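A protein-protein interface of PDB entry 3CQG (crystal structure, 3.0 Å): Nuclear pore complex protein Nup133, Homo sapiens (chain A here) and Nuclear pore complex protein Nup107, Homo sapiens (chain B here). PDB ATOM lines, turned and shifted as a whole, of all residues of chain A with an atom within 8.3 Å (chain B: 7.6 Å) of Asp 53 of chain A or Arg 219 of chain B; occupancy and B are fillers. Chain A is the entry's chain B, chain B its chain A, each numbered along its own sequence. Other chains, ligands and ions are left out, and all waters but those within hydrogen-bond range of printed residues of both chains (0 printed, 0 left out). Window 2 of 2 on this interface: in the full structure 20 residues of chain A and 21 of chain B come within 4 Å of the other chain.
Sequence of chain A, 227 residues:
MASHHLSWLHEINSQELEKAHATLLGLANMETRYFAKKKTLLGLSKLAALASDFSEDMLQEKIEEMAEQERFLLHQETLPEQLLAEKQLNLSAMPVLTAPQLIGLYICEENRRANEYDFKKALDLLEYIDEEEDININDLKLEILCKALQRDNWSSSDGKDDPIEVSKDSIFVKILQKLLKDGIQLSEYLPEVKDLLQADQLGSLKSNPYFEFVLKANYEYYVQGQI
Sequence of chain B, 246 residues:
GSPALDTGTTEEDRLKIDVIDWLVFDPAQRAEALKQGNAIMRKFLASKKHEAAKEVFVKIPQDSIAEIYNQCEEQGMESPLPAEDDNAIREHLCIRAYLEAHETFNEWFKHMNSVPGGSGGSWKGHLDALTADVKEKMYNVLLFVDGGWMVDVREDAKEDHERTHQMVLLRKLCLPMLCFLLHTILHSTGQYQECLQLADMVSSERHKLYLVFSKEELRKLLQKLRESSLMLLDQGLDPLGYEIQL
The guanidinium group (NH2) of Arg 219 of chain B lies within hydrogen-bond range of the backbone carbonyl oxygen (O) of Ala 51 of chain A (3.2 Å).
OD2 of Asp 53 of chain A is in salt-bridge range of NH2 of Arg 219 of chain B (3.6 Å).
Of the 14 printed residues of chain B, 6 touch a printed residue of chain A.
Along chain B the printed residues that touch a printed residue of chain A span positions 215 to 223.
Of the 17 printed residues of chain A, 7 touch a printed residue of chain B.
Printed residues of chain A that touch a printed residue of chain B: Ile 12, Leu 17, Leu 47, Leu 50, Ala 51, Ser 52 and Asp 53.
Hydrophobic or aromatic side chains of chain A within 4 Å of the printed part of chain B: Leu 17, Leu 47, Leu 50 and Ala 51.
Among the printed residues, 11 pairs touch across the chains.
Among the printed residues, Asp or Glu carboxylates within 4 Å of a Lys or Arg side-chain nitrogen of the other chain: Asp 53 of chain A with Arg 219 of chain B.
NE2 of Gln 223 of chain B touches O of Ile 12 of chain A, at 3.6 Å.
Leu 17 of chain A touches Arg 219 of chain B.
CD1 of Leu 47 of chain A touches CD2 of Leu 221 of chain B (3.8 Å).
Leu 47 of chain A touches Leu 222 of chain B (CB to CD2, 3.9 Å).
Leu 50 of chain A touches Lys 215 of chain B (O to CE, 3.2 Å).
Leu 50 of chain A touches Leu 218 of chain B (CB to CD1, 3.8 Å).
CB of Ala 51 of chain A touches CB of Leu 218 of chain B (3.4 Å).
Ala 51 of chain A touches Leu 222 of chain B (CB to CD1, 3.8 Å).
O of Ser 52 of chain A touches CE of Lys 215 of chain B (3.1 Å).
Of chain A, only Leu 17 (3.7 Å), Ala 51 (3.2 Å) and Asp 53 (3.6 Å) come within 4 Å of Arg 219 of chain B.
Of the printed residues of chain B, Ser 52 of chain A touches Lys 215 (3.1 Å).
Printed residues of chain A within 4 Å of Leu 221 of chain B: Leu 47 (3.8 Å).
Of the printed residues of chain B, Leu 17 of chain A touches Arg 219 (3.7 Å).
Printed residues of chain A within 4 Å of Leu 218 of chain B: Leu 50 (3.8 Å) and Ala 51 (3.4 Å).
Leu 225 of chain B touches none of the printed residues of chain A.
The nearest residue of chain B that does not touch Asp 53 of chain A is Lys 215 of chain B (5.2 Å).
The nearest residue of chain A that does not touch Arg 219 of chain B is Ser 52 of chain A (4.3 Å).
The nearest printed residue of chain B that does not touch Ala 51 of chain A is Lys 215 of chain B (4.2 Å).
NH1 of Arg 219 of chain B lies within salt-bridge range of OE2 of Glu 216 of chain B (3.7 Å).
OE2 of Glu 18 of chain A is in hydrogen-bond range of N of Asp 53 of chain A, 3.4 Å away.
OG of Ser 52 of chain A lies close to O of Ala 48 of chain A, 3.4 Å away.
O of Ala 49 of chain A sits at hydrogen-bond distance from OG of Ser 52 of chain A, at 2.6 Å.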
ATOM      1  N   ILE A  12     -26.357   7.002   5.347  1.00  0.00           N
ATOM      2  CA  ILE A  12     -25.998   6.039   4.324  1.00  0.00           C
ATOM      3  C   ILE A  12     -24.541   6.187   3.910  1.00  0.00           C
ATOM      4  O   ILE A  12     -23.791   5.209   3.893  1.00  0.00           O
ATOM      5  CB  ILE A  12     -26.877   6.177   3.081  1.00  0.00           C
ATOM      6  CG1 ILE A  12     -28.308   5.743   3.385  1.00  0.00           C
ATOM      7  CG2 ILE A  12     -26.322   5.334   1.951  1.00  0.00           C
ATOM      8  CD1 ILE A  12     -29.218   5.825   2.180  1.00  0.00           C
ATOM      9  N   GLN A  15     -22.214   4.580   6.080  1.00  0.00           N
ATOM     10  CA  GLN A  15     -22.407   3.144   6.293  1.00  0.00           C
ATOM     11  C   GLN A  15     -23.146   2.819   7.597  1.00  0.00           C
ATOM     12  O   GLN A  15     -23.102   1.682   8.080  1.00  0.00           O
ATOM     13  CB  GLN A  15     -21.080   2.376   6.216  1.00  0.00           C
ATOM     14  CG  GLN A  15     -20.419   2.376   4.844  1.00  0.00           C
ATOM     15  CD  GLN A  15     -19.425   3.515   4.667  1.00  0.00           C
ATOM     16  OE1 GLN A  15     -19.234   4.328   5.570  1.00  0.00           O
ATOM     17  NE2 GLN A  15     -18.781   3.572   3.502  1.00  0.00           N
ATOM     18  N   GLU A  16     -23.821   3.816   8.159  1.00  0.00           N
ATOM     19  CA  GLU A  16     -24.696   3.585   9.296  1.00  0.00           C
ATOM     20  C   GLU A  16     -26.058   3.196   8.750  1.00  0.00           C
ATOM     21  O   GLU A  16     -26.965   4.027   8.669  1.00  0.00           O
ATOM     22  CB  GLU A  16     -24.823   4.849  10.138  1.00  0.00           C
ATOM     23  CG  GLU A  16     -23.494   5.456  10.561  1.00  0.00           C
ATOM     24  CD  GLU A  16     -23.621   6.927  10.926  1.00  0.00           C
ATOM     25  OE1 GLU A  16     -24.764   7.431  11.007  1.00  0.00           O
ATOM     26  OE2 GLU A  16     -22.576   7.582  11.125  1.00  0.00           O
ATOM     27  N   LEU A  17     -26.198   1.931   8.370  1.00  0.00           N
ATOM     28  CA  LEU A  17     -27.383   1.483   7.646  1.00  0.00           C
ATOM     29  C   LEU A  17     -28.495   0.999   8.565  1.00  0.00           C
ATOM     30  O   LEU A  17     -29.660   1.009   8.185  1.00  0.00           O
ATOM     31  CB  LEU A  17     -27.010   0.412   6.624  1.00  0.00           C
ATOM     32  CG  LEU A  17     -25.911   0.829   5.647  1.00  0.00           C
ATOM     33  CD1 LEU A  17     -25.440  -0.374   4.868  1.00  0.00           C
ATOM     34  CD2 LEU A  17     -26.380   1.936   4.719  1.00  0.00           C
ATOM     35  N   GLU A  18     -28.138   0.577   9.774  1.00  0.00           N
ATOM     36  CA  GLU A  18     -29.142   0.342  10.801  1.00  0.00           C
ATOM     37  C   GLU A  18     -29.844   1.655  11.087  1.00  0.00           C
ATOM     38  O   GLU A  18     -31.036   1.679  11.386  1.00  0.00           O
ATOM     39  CB  GLU A  18     -28.515  -0.189  12.094  1.00  0.00           C
ATOM     40  CG  GLU A  18     -28.014  -1.624  12.012  1.00  0.00           C
ATOM     41  CD  GLU A  18     -26.501  -1.721  11.893  1.00  0.00           C
ATOM     42  OE1 GLU A  18     -25.830  -1.682  12.945  1.00  0.00           O
ATOM     43  OE2 GLU A  18     -25.982  -1.866  10.762  1.00  0.00           O
ATOM     44  N   LEU A  47     -34.315  -2.005   1.995  1.00  0.00           N
ATOM     45  CA  LEU A  47     -32.989  -2.257   1.443  1.00  0.00           C
ATOM     46  C   LEU A  47     -31.911  -1.999   2.482  1.00  0.00           C
ATOM     47  O   LEU A  47     -30.996  -2.801   2.652  1.00  0.00           O
ATOM     48  CB  LEU A  47     -32.735  -1.394   0.209  1.00  0.00           C
ATOM     49  CG  LEU A  47     -33.602  -1.695  -1.012  1.00  0.00           C
ATOM     50  CD1 LEU A  47     -33.022  -1.021  -2.250  1.00  0.00           C
ATOM     51  CD2 LEU A  47     -33.749  -3.200  -1.233  1.00  0.00           C
ATOM     52  N   ALA A  48     -32.023  -0.868   3.172  1.00  0.00           N
ATOM     53  CA  ALA A  48     -31.089  -0.517   4.234  1.00  0.00           C
ATOM     54  C   ALA A  48     -30.997  -1.628   5.290  1.00  0.00           C
ATOM     55  O   ALA A  48     -29.911  -2.091   5.629  1.00  0.00           O
ATOM     56  CB  ALA A  48     -31.499   0.810   4.869  1.00  0.00           C
ATOM     57  N   ALA A  49     -32.151  -2.051   5.795  1.00  0.00           N
ATOM     58  CA  ALA A  49     -32.232  -3.145   6.753  1.00  0.00           C
ATOM     59  C   ALA A  49     -31.512  -4.391   6.241  1.00  0.00           C
ATOM     60  O   ALA A  49     -30.691  -4.979   6.946  1.00  0.00           O
ATOM     61  CB  ALA A  49     -33.684  -3.461   7.051  1.00  0.00           C
ATOM     62  N   LEU A  50     -31.830  -4.788   5.012  1.00  0.00           N
ATOM     63  CA  LEU A  50     -31.238  -5.966   4.391  1.00  0.00           C
ATOM     64  C   LEU A  50     -29.732  -5.854   4.217  1.00  0.00           C
ATOM     65  O   LEU A  50     -29.010  -6.834   4.369  1.00  0.00           O
ATOM     66  CB  LEU A  50     -31.869  -6.212   3.026  1.00  0.00           C
ATOM     67  CG  LEU A  50     -33.187  -6.968   2.993  1.00  0.00           C
ATOM     68  CD1 LEU A  50     -33.784  -6.826   1.620  1.00  0.00           C
ATOM     69  CD2 LEU A  50     -32.975  -8.432   3.337  1.00  0.00           C
ATOM     70  N   ALA A  51     -29.267  -4.655   3.885  1.00  0.00           N
ATOM     71  CA  ALA A  51     -27.864  -4.436   3.553  1.00  0.00           C
ATOM     72  C   ALA A  51     -27.036  -4.037   4.762  1.00  0.00           C
ATOM     73  O   ALA A  51     -25.849  -3.739   4.638  1.00  0.00           O
ATOM     74  CB  ALA A  51     -27.742  -3.382   2.479  1.00  0.00           C
ATOM     75  N   SER A  52     -27.663  -4.018   5.931  1.00  0.00           N
ATOM     76  CA  SER A  52     -26.955  -3.678   7.155  1.00  0.00           C
ATOM     77  C   SER A  52     -26.414  -4.929   7.833  1.00  0.00           C
ATOM     78  O   SER A  52     -26.353  -6.004   7.230  1.00  0.00           O
ATOM     79  CB  SER A  52     -27.879  -2.935   8.111  1.00  0.00           C
ATOM     80  OG  SER A  52     -28.994  -3.740   8.441  1.00  0.00           O
ATOM     81  N   ASP A  53     -26.035  -4.783   9.098  1.00  0.00           N
ATOM     82  CA  ASP A  53     -25.429  -5.873   9.848  1.00  0.00           C
ATOM     83  C   ASP A  53     -26.339  -6.312  11.005  1.00  0.00           C
ATOM     84  O   ASP A  53     -25.860  -6.690  12.076  1.00  0.00           O
ATOM     85  CB  ASP A  53     -24.035  -5.467  10.361  1.00  0.00           C
ATOM     86  CG  ASP A  53     -23.237  -4.624   9.346  1.00  0.00           C
ATOM     87  OD1 ASP A  53     -22.095  -5.008   9.007  1.00  0.00           O
ATOM     88  OD2 ASP A  53     -23.741  -3.567   8.900  1.00  0.00           O
ATOM     89  N   PHE A  54     -27.649  -6.257  10.782  1.00  0.00           N
ATOM     90  CA  PHE A  54     -28.612  -6.635  11.806  1.00  0.00           C
ATOM     91  C   PHE A  54     -28.457  -8.111  12.136  1.00  0.00           C
ATOM     92  O   PHE A  54     -27.904  -8.870  11.345  1.00  0.00           O
ATOM     93  CB  PHE A  54     -30.047  -6.335  11.353  1.00  0.00           C
ATOM     94  CG  PHE A  54     -30.504  -4.933  11.659  1.00  0.00           C
ATOM     95  CD1 PHE A  54     -30.344  -4.402  12.929  1.00  0.00           C
ATOM     96  CD2 PHE A  54     -31.107  -4.152  10.685  1.00  0.00           C
ATOM     97  CE1 PHE A  54     -30.761  -3.118  13.218  1.00  0.00           C
ATOM     98  CE2 PHE A  54     -31.527  -2.864  10.970  1.00  0.00           C
ATOM     99  CZ  PHE A  54     -31.356  -2.347  12.240  1.00  0.00           C
ATOM    100  N   SER A  55     -28.929  -8.515  13.311  1.00  0.00           N
ATOM    101  CA  SER A  55     -28.872  -9.918  13.698  1.00  0.00           C
ATOM    102  C   SER A  55     -29.753 -10.753  12.776  1.00  0.00           C
ATOM    103  O   SER A  55     -30.784 -10.285  12.297  1.00  0.00           O
ATOM    104  CB  SER A  55     -29.302 -10.095  15.152  1.00  0.00           C
ATOM    105  OG  SER A  55     -29.463 -11.467  15.464  1.00  0.00           O
ATOM    106  N   GLU A  56     -29.347 -11.994  12.532  1.00  0.00           N
ATOM    107  CA  GLU A  56     -30.065 -12.864  11.608  1.00  0.00           C
ATOM    108  C   GLU A  56     -31.540 -13.015  11.989  1.00  0.00           C
ATOM    109  O   GLU A  56     -32.358 -13.460  11.182  1.00  0.00           O
ATOM    110  CB  GLU A  56     -29.365 -14.225  11.519  1.00  0.00           C
ATOM    111  CG  GLU A  56     -29.998 -15.206  10.545  1.00  0.00           C
ATOM    112  CD  GLU A  56     -28.984 -16.124   9.881  1.00  0.00           C
ATOM    113  OE1 GLU A  56     -27.783 -16.039  10.211  1.00  0.00           O
ATOM    114  OE2 GLU A  56     -29.394 -16.928   9.018  1.00  0.00           O
ATOM    115  N   MET A  58     -33.045 -10.403  14.375  1.00  0.00           N
ATOM    116  CA  MET A  58     -33.360  -8.982  14.432  1.00  0.00           C
ATOM    117  C   MET A  58     -33.737  -8.494  13.038  1.00  0.00           C
ATOM    118  O   MET A  58     -34.695  -7.738  12.867  1.00  0.00           O
ATOM    119  CB  MET A  58     -32.135  -8.224  14.942  1.00  0.00           C
ATOM    120  CG  MET A  58     -32.369  -6.791  15.362  1.00  0.00           C
ATOM    121  SD  MET A  58     -30.900  -6.159  16.213  1.00  0.00           S
ATOM    122  CE  MET A  58     -30.764  -7.342  17.555  1.00  0.00           C
ATOM    123  N   LEU A  59     -32.966  -8.930  12.047  1.00  0.00           N
ATOM    124  CA  LEU A  59     -33.268  -8.661  10.649  1.00  0.00           C
ATOM    125  C   LEU A  59     -34.587  -9.305  10.255  1.00  0.00           C
ATOM    126  O   LEU A  59     -35.544  -8.615   9.933  1.00  0.00           O
ATOM    127  CB  LEU A  59     -32.154  -9.201   9.754  1.00  0.00           C
ATOM    128  CG  LEU A  59     -32.484  -9.314   8.267  1.00  0.00           C
ATOM    129  CD1 LEU A  59     -32.594  -7.945   7.613  1.00  0.00           C
ATOM    130  CD2 LEU A  59     -31.441 -10.154   7.566  1.00  0.00           C
ATOM    131  N   PHE B 180     -27.572  -2.472 -12.128  1.00  0.00           N
ATOM    132  CA  PHE B 180     -26.625  -1.366 -12.085  1.00  0.00           C
ATOM    133  C   PHE B 180     -26.511  -0.701 -13.442  1.00  0.00           C
ATOM    134  O   PHE B 180     -26.375   0.501 -13.542  1.00  0.00           O
ATOM    135  CB  PHE B 180     -25.257  -1.841 -11.603  1.00  0.00           C
ATOM    136  CG  PHE B 180     -25.265  -2.431 -10.215  1.00  0.00           C
ATOM    137  CD1 PHE B 180     -25.930  -1.805  -9.170  1.00  0.00           C
ATOM    138  CD2 PHE B 180     -24.574  -3.594  -9.955  1.00  0.00           C
ATOM    139  CE1 PHE B 180     -25.920  -2.348  -7.897  1.00  0.00           C
ATOM    140  CE2 PHE B 180     -24.555  -4.142  -8.697  1.00  0.00           C
ATOM    141  CZ  PHE B 180     -25.234  -3.518  -7.658  1.00  0.00           C
ATOM    142  N   PHE B 213     -29.299 -10.474  -4.268  1.00  0.00           N
ATOM    143  CA  PHE B 213     -28.226  -9.496  -4.081  1.00  0.00           C
ATOM    144  C   PHE B 213     -27.367  -9.874  -2.869  1.00  0.00           C
ATOM    145  O   PHE B 213     -27.882 -10.313  -1.839  1.00  0.00           O
ATOM    146  CB  PHE B 213     -28.805  -8.107  -3.806  1.00  0.00           C
ATOM    147  CG  PHE B 213     -29.107  -7.286  -5.033  1.00  0.00           C
ATOM    148  CD1 PHE B 213     -30.232  -7.549  -5.814  1.00  0.00           C
ATOM    149  CD2 PHE B 213     -28.301  -6.203  -5.372  1.00  0.00           C
ATOM    150  CE1 PHE B 213     -30.527  -6.771  -6.926  1.00  0.00           C
ATOM    151  CE2 PHE B 213     -28.592  -5.421  -6.488  1.00  0.00           C
ATOM    152  CZ  PHE B 213     -29.708  -5.706  -7.260  1.00  0.00           C
ATOM    153  N   SER B 214     -26.058  -9.694  -2.994  1.00  0.00           N
ATOM    154  CA  SER B 214     -25.164  -9.787  -1.851  1.00  0.00           C
ATOM    155  C   SER B 214     -25.224  -8.470  -1.107  1.00  0.00           C
ATOM    156  O   SER B 214     -25.563  -7.445  -1.685  1.00  0.00           O
ATOM    157  CB  SER B 214     -23.731 -10.004  -2.310  1.00  0.00           C
ATOM    158  OG  SER B 214     -23.157  -8.770  -2.691  1.00  0.00           O
ATOM    159  N   LYS B 215     -24.871  -8.485   0.172  1.00  0.00           N
ATOM    160  CA  LYS B 215     -24.882  -7.254   0.951  1.00  0.00           C
ATOM    161  C   LYS B 215     -23.945  -6.216   0.345  1.00  0.00           C
ATOM    162  O   LYS B 215     -24.166  -5.021   0.484  1.00  0.00           O
ATOM    163  CB  LYS B 215     -24.535  -7.518   2.417  1.00  0.00           C
ATOM    164  CG  LYS B 215     -25.654  -8.172   3.212  1.00  0.00           C
ATOM    165  CD  LYS B 215     -25.495  -7.904   4.703  1.00  0.00           C
ATOM    166  CE  LYS B 215     -26.583  -8.589   5.532  1.00  0.00           C
ATOM    167  NZ  LYS B 215     -26.319 -10.043   5.747  1.00  0.00           N
ATOM    168  N   GLU B 216     -22.905  -6.684  -0.335  1.00  0.00           N
ATOM    169  CA  GLU B 216     -21.962  -5.796  -0.990  1.00  0.00           C
ATOM    170  C   GLU B 216     -22.646  -5.036  -2.101  1.00  0.00           C
ATOM    171  O   GLU B 216     -22.389  -3.852  -2.303  1.00  0.00           O
ATOM    172  CB  GLU B 216     -20.815  -6.596  -1.596  1.00  0.00           C
ATOM    173  CG  GLU B 216     -19.471  -6.105  -1.158  1.00  0.00           C
ATOM    174  CD  GLU B 216     -19.259  -6.334   0.325  1.00  0.00           C
ATOM    175  OE1 GLU B 216     -19.374  -7.501   0.765  1.00  0.00           O
ATOM    176  OE2 GLU B 216     -18.983  -5.350   1.052  1.00  0.00           O
ATOM    177  N   GLU B 217     -23.514  -5.735  -2.824  1.00  0.00           N
ATOM    178  CA  GLU B 217     -24.185  -5.176  -3.989  1.00  0.00           C
ATOM    179  C   GLU B 217     -25.347  -4.271  -3.584  1.00  0.00           C
ATOM    180  O   GLU B 217     -25.623  -3.267  -4.245  1.00  0.00           O
ATOM    181  CB  GLU B 217     -24.667  -6.304  -4.891  1.00  0.00           C
ATOM    182  CG  GLU B 217     -23.624  -7.389  -5.057  1.00  0.00           C
ATOM    183  CD  GLU B 217     -23.994  -8.411  -6.108  1.00  0.00           C
ATOM    184  OE1 GLU B 217     -24.966  -9.165  -5.881  1.00  0.00           O
ATOM    185  OE2 GLU B 217     -23.300  -8.467  -7.150  1.00  0.00           O
ATOM    186  N   LEU B 218     -26.015  -4.631  -2.490  1.00  0.00           N
ATOM    187  CA  LEU B 218     -27.104  -3.835  -1.942  1.00  0.00           C
ATOM    188  C   LEU B 218     -26.559  -2.495  -1.496  1.00  0.00           C
ATOM    189  O   LEU B 218     -27.204  -1.464  -1.642  1.00  0.00           O
ATOM    190  CB  LEU B 218     -27.757  -4.551  -0.760  1.00  0.00           C
ATOM    191  CG  LEU B 218     -28.842  -5.574  -1.093  1.00  0.00           C
ATOM    192  CD1 LEU B 218     -29.445  -6.182   0.159  1.00  0.00           C
ATOM    193  CD2 LEU B 218     -29.917  -4.923  -1.937  1.00  0.00           C
ATOM    194  N   ARG B 219     -25.357  -2.515  -0.945  1.00  0.00           N
ATOM    195  CA  ARG B 219     -24.709  -1.294  -0.521  1.00  0.00           C
ATOM    196  C   ARG B 219     -24.364  -0.495  -1.761  1.00  0.00           C
ATOM    197  O   ARG B 219     -24.711   0.673  -1.878  1.00  0.00           O
ATOM    198  CB  ARG B 219     -23.453  -1.610   0.297  1.00  0.00           C
ATOM    199  CG  ARG B 219     -23.746  -2.313   1.609  1.00  0.00           C
ATOM    200  CD  ARG B 219     -22.512  -2.377   2.478  1.00  0.00           C
ATOM    201  NE  ARG B 219     -22.830  -2.848   3.818  1.00  0.00           N
ATOM    202  CZ  ARG B 219     -22.450  -4.023   4.308  1.00  0.00           C
ATOM    203  NH1 ARG B 219     -21.717  -4.849   3.567  1.00  0.00           N
ATOM    204  NH2 ARG B 219     -22.795  -4.367   5.544  1.00  0.00           N
ATOM    205  N   LYS B 220     -23.695  -1.139  -2.701  1.00  0.00           N
ATOM    206  CA  LYS B 220     -23.332  -0.470  -3.925  1.00  0.00           C
ATOM    207  C   LYS B 220     -24.570   0.210  -4.473  1.00  0.00           C
ATOM    208  O   LYS B 220     -24.518   1.363  -4.884  1.00  0.00           O
ATOM    209  CB  LYS B 220     -22.775  -1.482  -4.923  1.00  0.00           C
ATOM    210  CG  LYS B 220     -22.061  -0.873  -6.115  1.00  0.00           C
ATOM    211  CD  LYS B 220     -21.663  -1.949  -7.119  1.00  0.00           C
ATOM    212  CE  LYS B 220     -20.822  -1.362  -8.252  1.00  0.00           C
ATOM    213  NZ  LYS B 220     -20.701  -2.284  -9.424  1.00  0.00           N
ATOM    214  N   LEU B 221     -25.692  -0.501  -4.452  1.00  0.00           N
ATOM    215  CA  LEU B 221     -26.939   0.019  -5.003  1.00  0.00           C
ATOM    216  C   LEU B 221     -27.409   1.247  -4.238  1.00  0.00           C
ATOM    217  O   LEU B 221     -27.717   2.273  -4.834  1.00  0.00           O
ATOM    218  CB  LEU B 221     -28.029  -1.055  -5.002  1.00  0.00           C
ATOM    219  CG  LEU B 221     -29.438  -0.623  -5.426  1.00  0.00           C
ATOM    220  CD1 LEU B 221     -29.517  -0.392  -6.928  1.00  0.00           C
ATOM    221  CD2 LEU B 221     -30.460  -1.651  -4.996  1.00  0.00           C
ATOM    222  N   LEU B 222     -27.447   1.138  -2.914  1.00  0.00           N
ATOM    223  CA  LEU B 222     -27.774   2.261  -2.034  1.00  0.00           C
ATOM    224  C   LEU B 222     -26.945   3.517  -2.298  1.00  0.00           C
ATOM    225  O   LEU B 222     -27.467   4.620  -2.334  1.00  0.00           O
ATOM    226  CB  LEU B 222     -27.576   1.839  -0.582  1.00  0.00           C
ATOM    227  CG  LEU B 222     -28.470   0.722  -0.048  1.00  0.00           C
ATOM    228  CD1 LEU B 222     -27.906   0.167   1.247  1.00  0.00           C
ATOM    229  CD2 LEU B 222     -29.877   1.244   0.148  1.00  0.00           C
ATOM    230  N   GLN B 223     -25.641   3.342  -2.453  1.00  0.00           N
ATOM    231  CA  GLN B 223     -24.735   4.465  -2.654  1.00  0.00           C
ATOM    232  C   GLN B 223     -24.927   5.139  -4.012  1.00  0.00           C
ATOM    233  O   GLN B 223     -24.729   6.345  -4.149  1.00  0.00           O
ATOM    234  CB  GLN B 223     -23.283   4.014  -2.499  1.00  0.00           C
ATOM    235  CG  GLN B 223     -23.009   3.143  -1.282  1.00  0.00           C
ATOM    236  CD  GLN B 223     -22.719   3.941  -0.021  1.00  0.00           C
ATOM    237  OE1 GLN B 223     -22.652   5.171  -0.058  1.00  0.00           O
ATOM    238  NE2 GLN B 223     -22.544   3.243   1.103  1.00  0.00           N
ATOM    239  N   LYS B 224     -25.282   4.346  -5.020  1.00  0.00           N
ATOM    240  CA  LYS B 224     -25.590   4.860  -6.358  1.00  0.00           C
ATOM    241  C   LYS B 224     -26.852   5.725  -6.377  1.00  0.00           C
ATOM    242  O   LYS B 224     -26.977   6.649  -7.170  1.00  0.00           O
ATOM    243  CB  LYS B 224     -25.774   3.700  -7.341  1.00  0.00           C
ATOM    244  CG  LYS B 224     -24.546   3.325  -8.110  1.00  0.00           C
ATOM    245  CD  LYS B 224     -24.775   2.059  -8.911  1.00  0.00           C
ATOM    246  CE  LYS B 224     -23.561   1.714  -9.762  1.00  0.00           C
ATOM    247  NZ  LYS B 224     -23.590   2.408 -11.081  1.00  0.00           N
ATOM    248  N   LEU B 225     -27.797   5.393  -5.509  1.00  0.00           N
ATOM    249  CA  LEU B 225     -29.073   6.085  -5.465  1.00  0.00           C
ATOM    250  C   LEU B 225     -28.920   7.384  -4.699  1.00  0.00           C
ATOM    251  O   LEU B 225     -29.665   8.347  -4.923  1.00  0.00           O
ATOM    252  CB  LEU B 225     -30.150   5.214  -4.811  1.00  0.00           C
ATOM    253  CG  LEU B 225     -30.504   3.916  -5.536  1.00  0.00           C
ATOM    254  CD1 LEU B 225     -31.760   3.283  -4.963  1.00  0.00           C
ATOM    255  CD2 LEU B 225     -30.662   4.173  -7.026  1.00  0.00           C
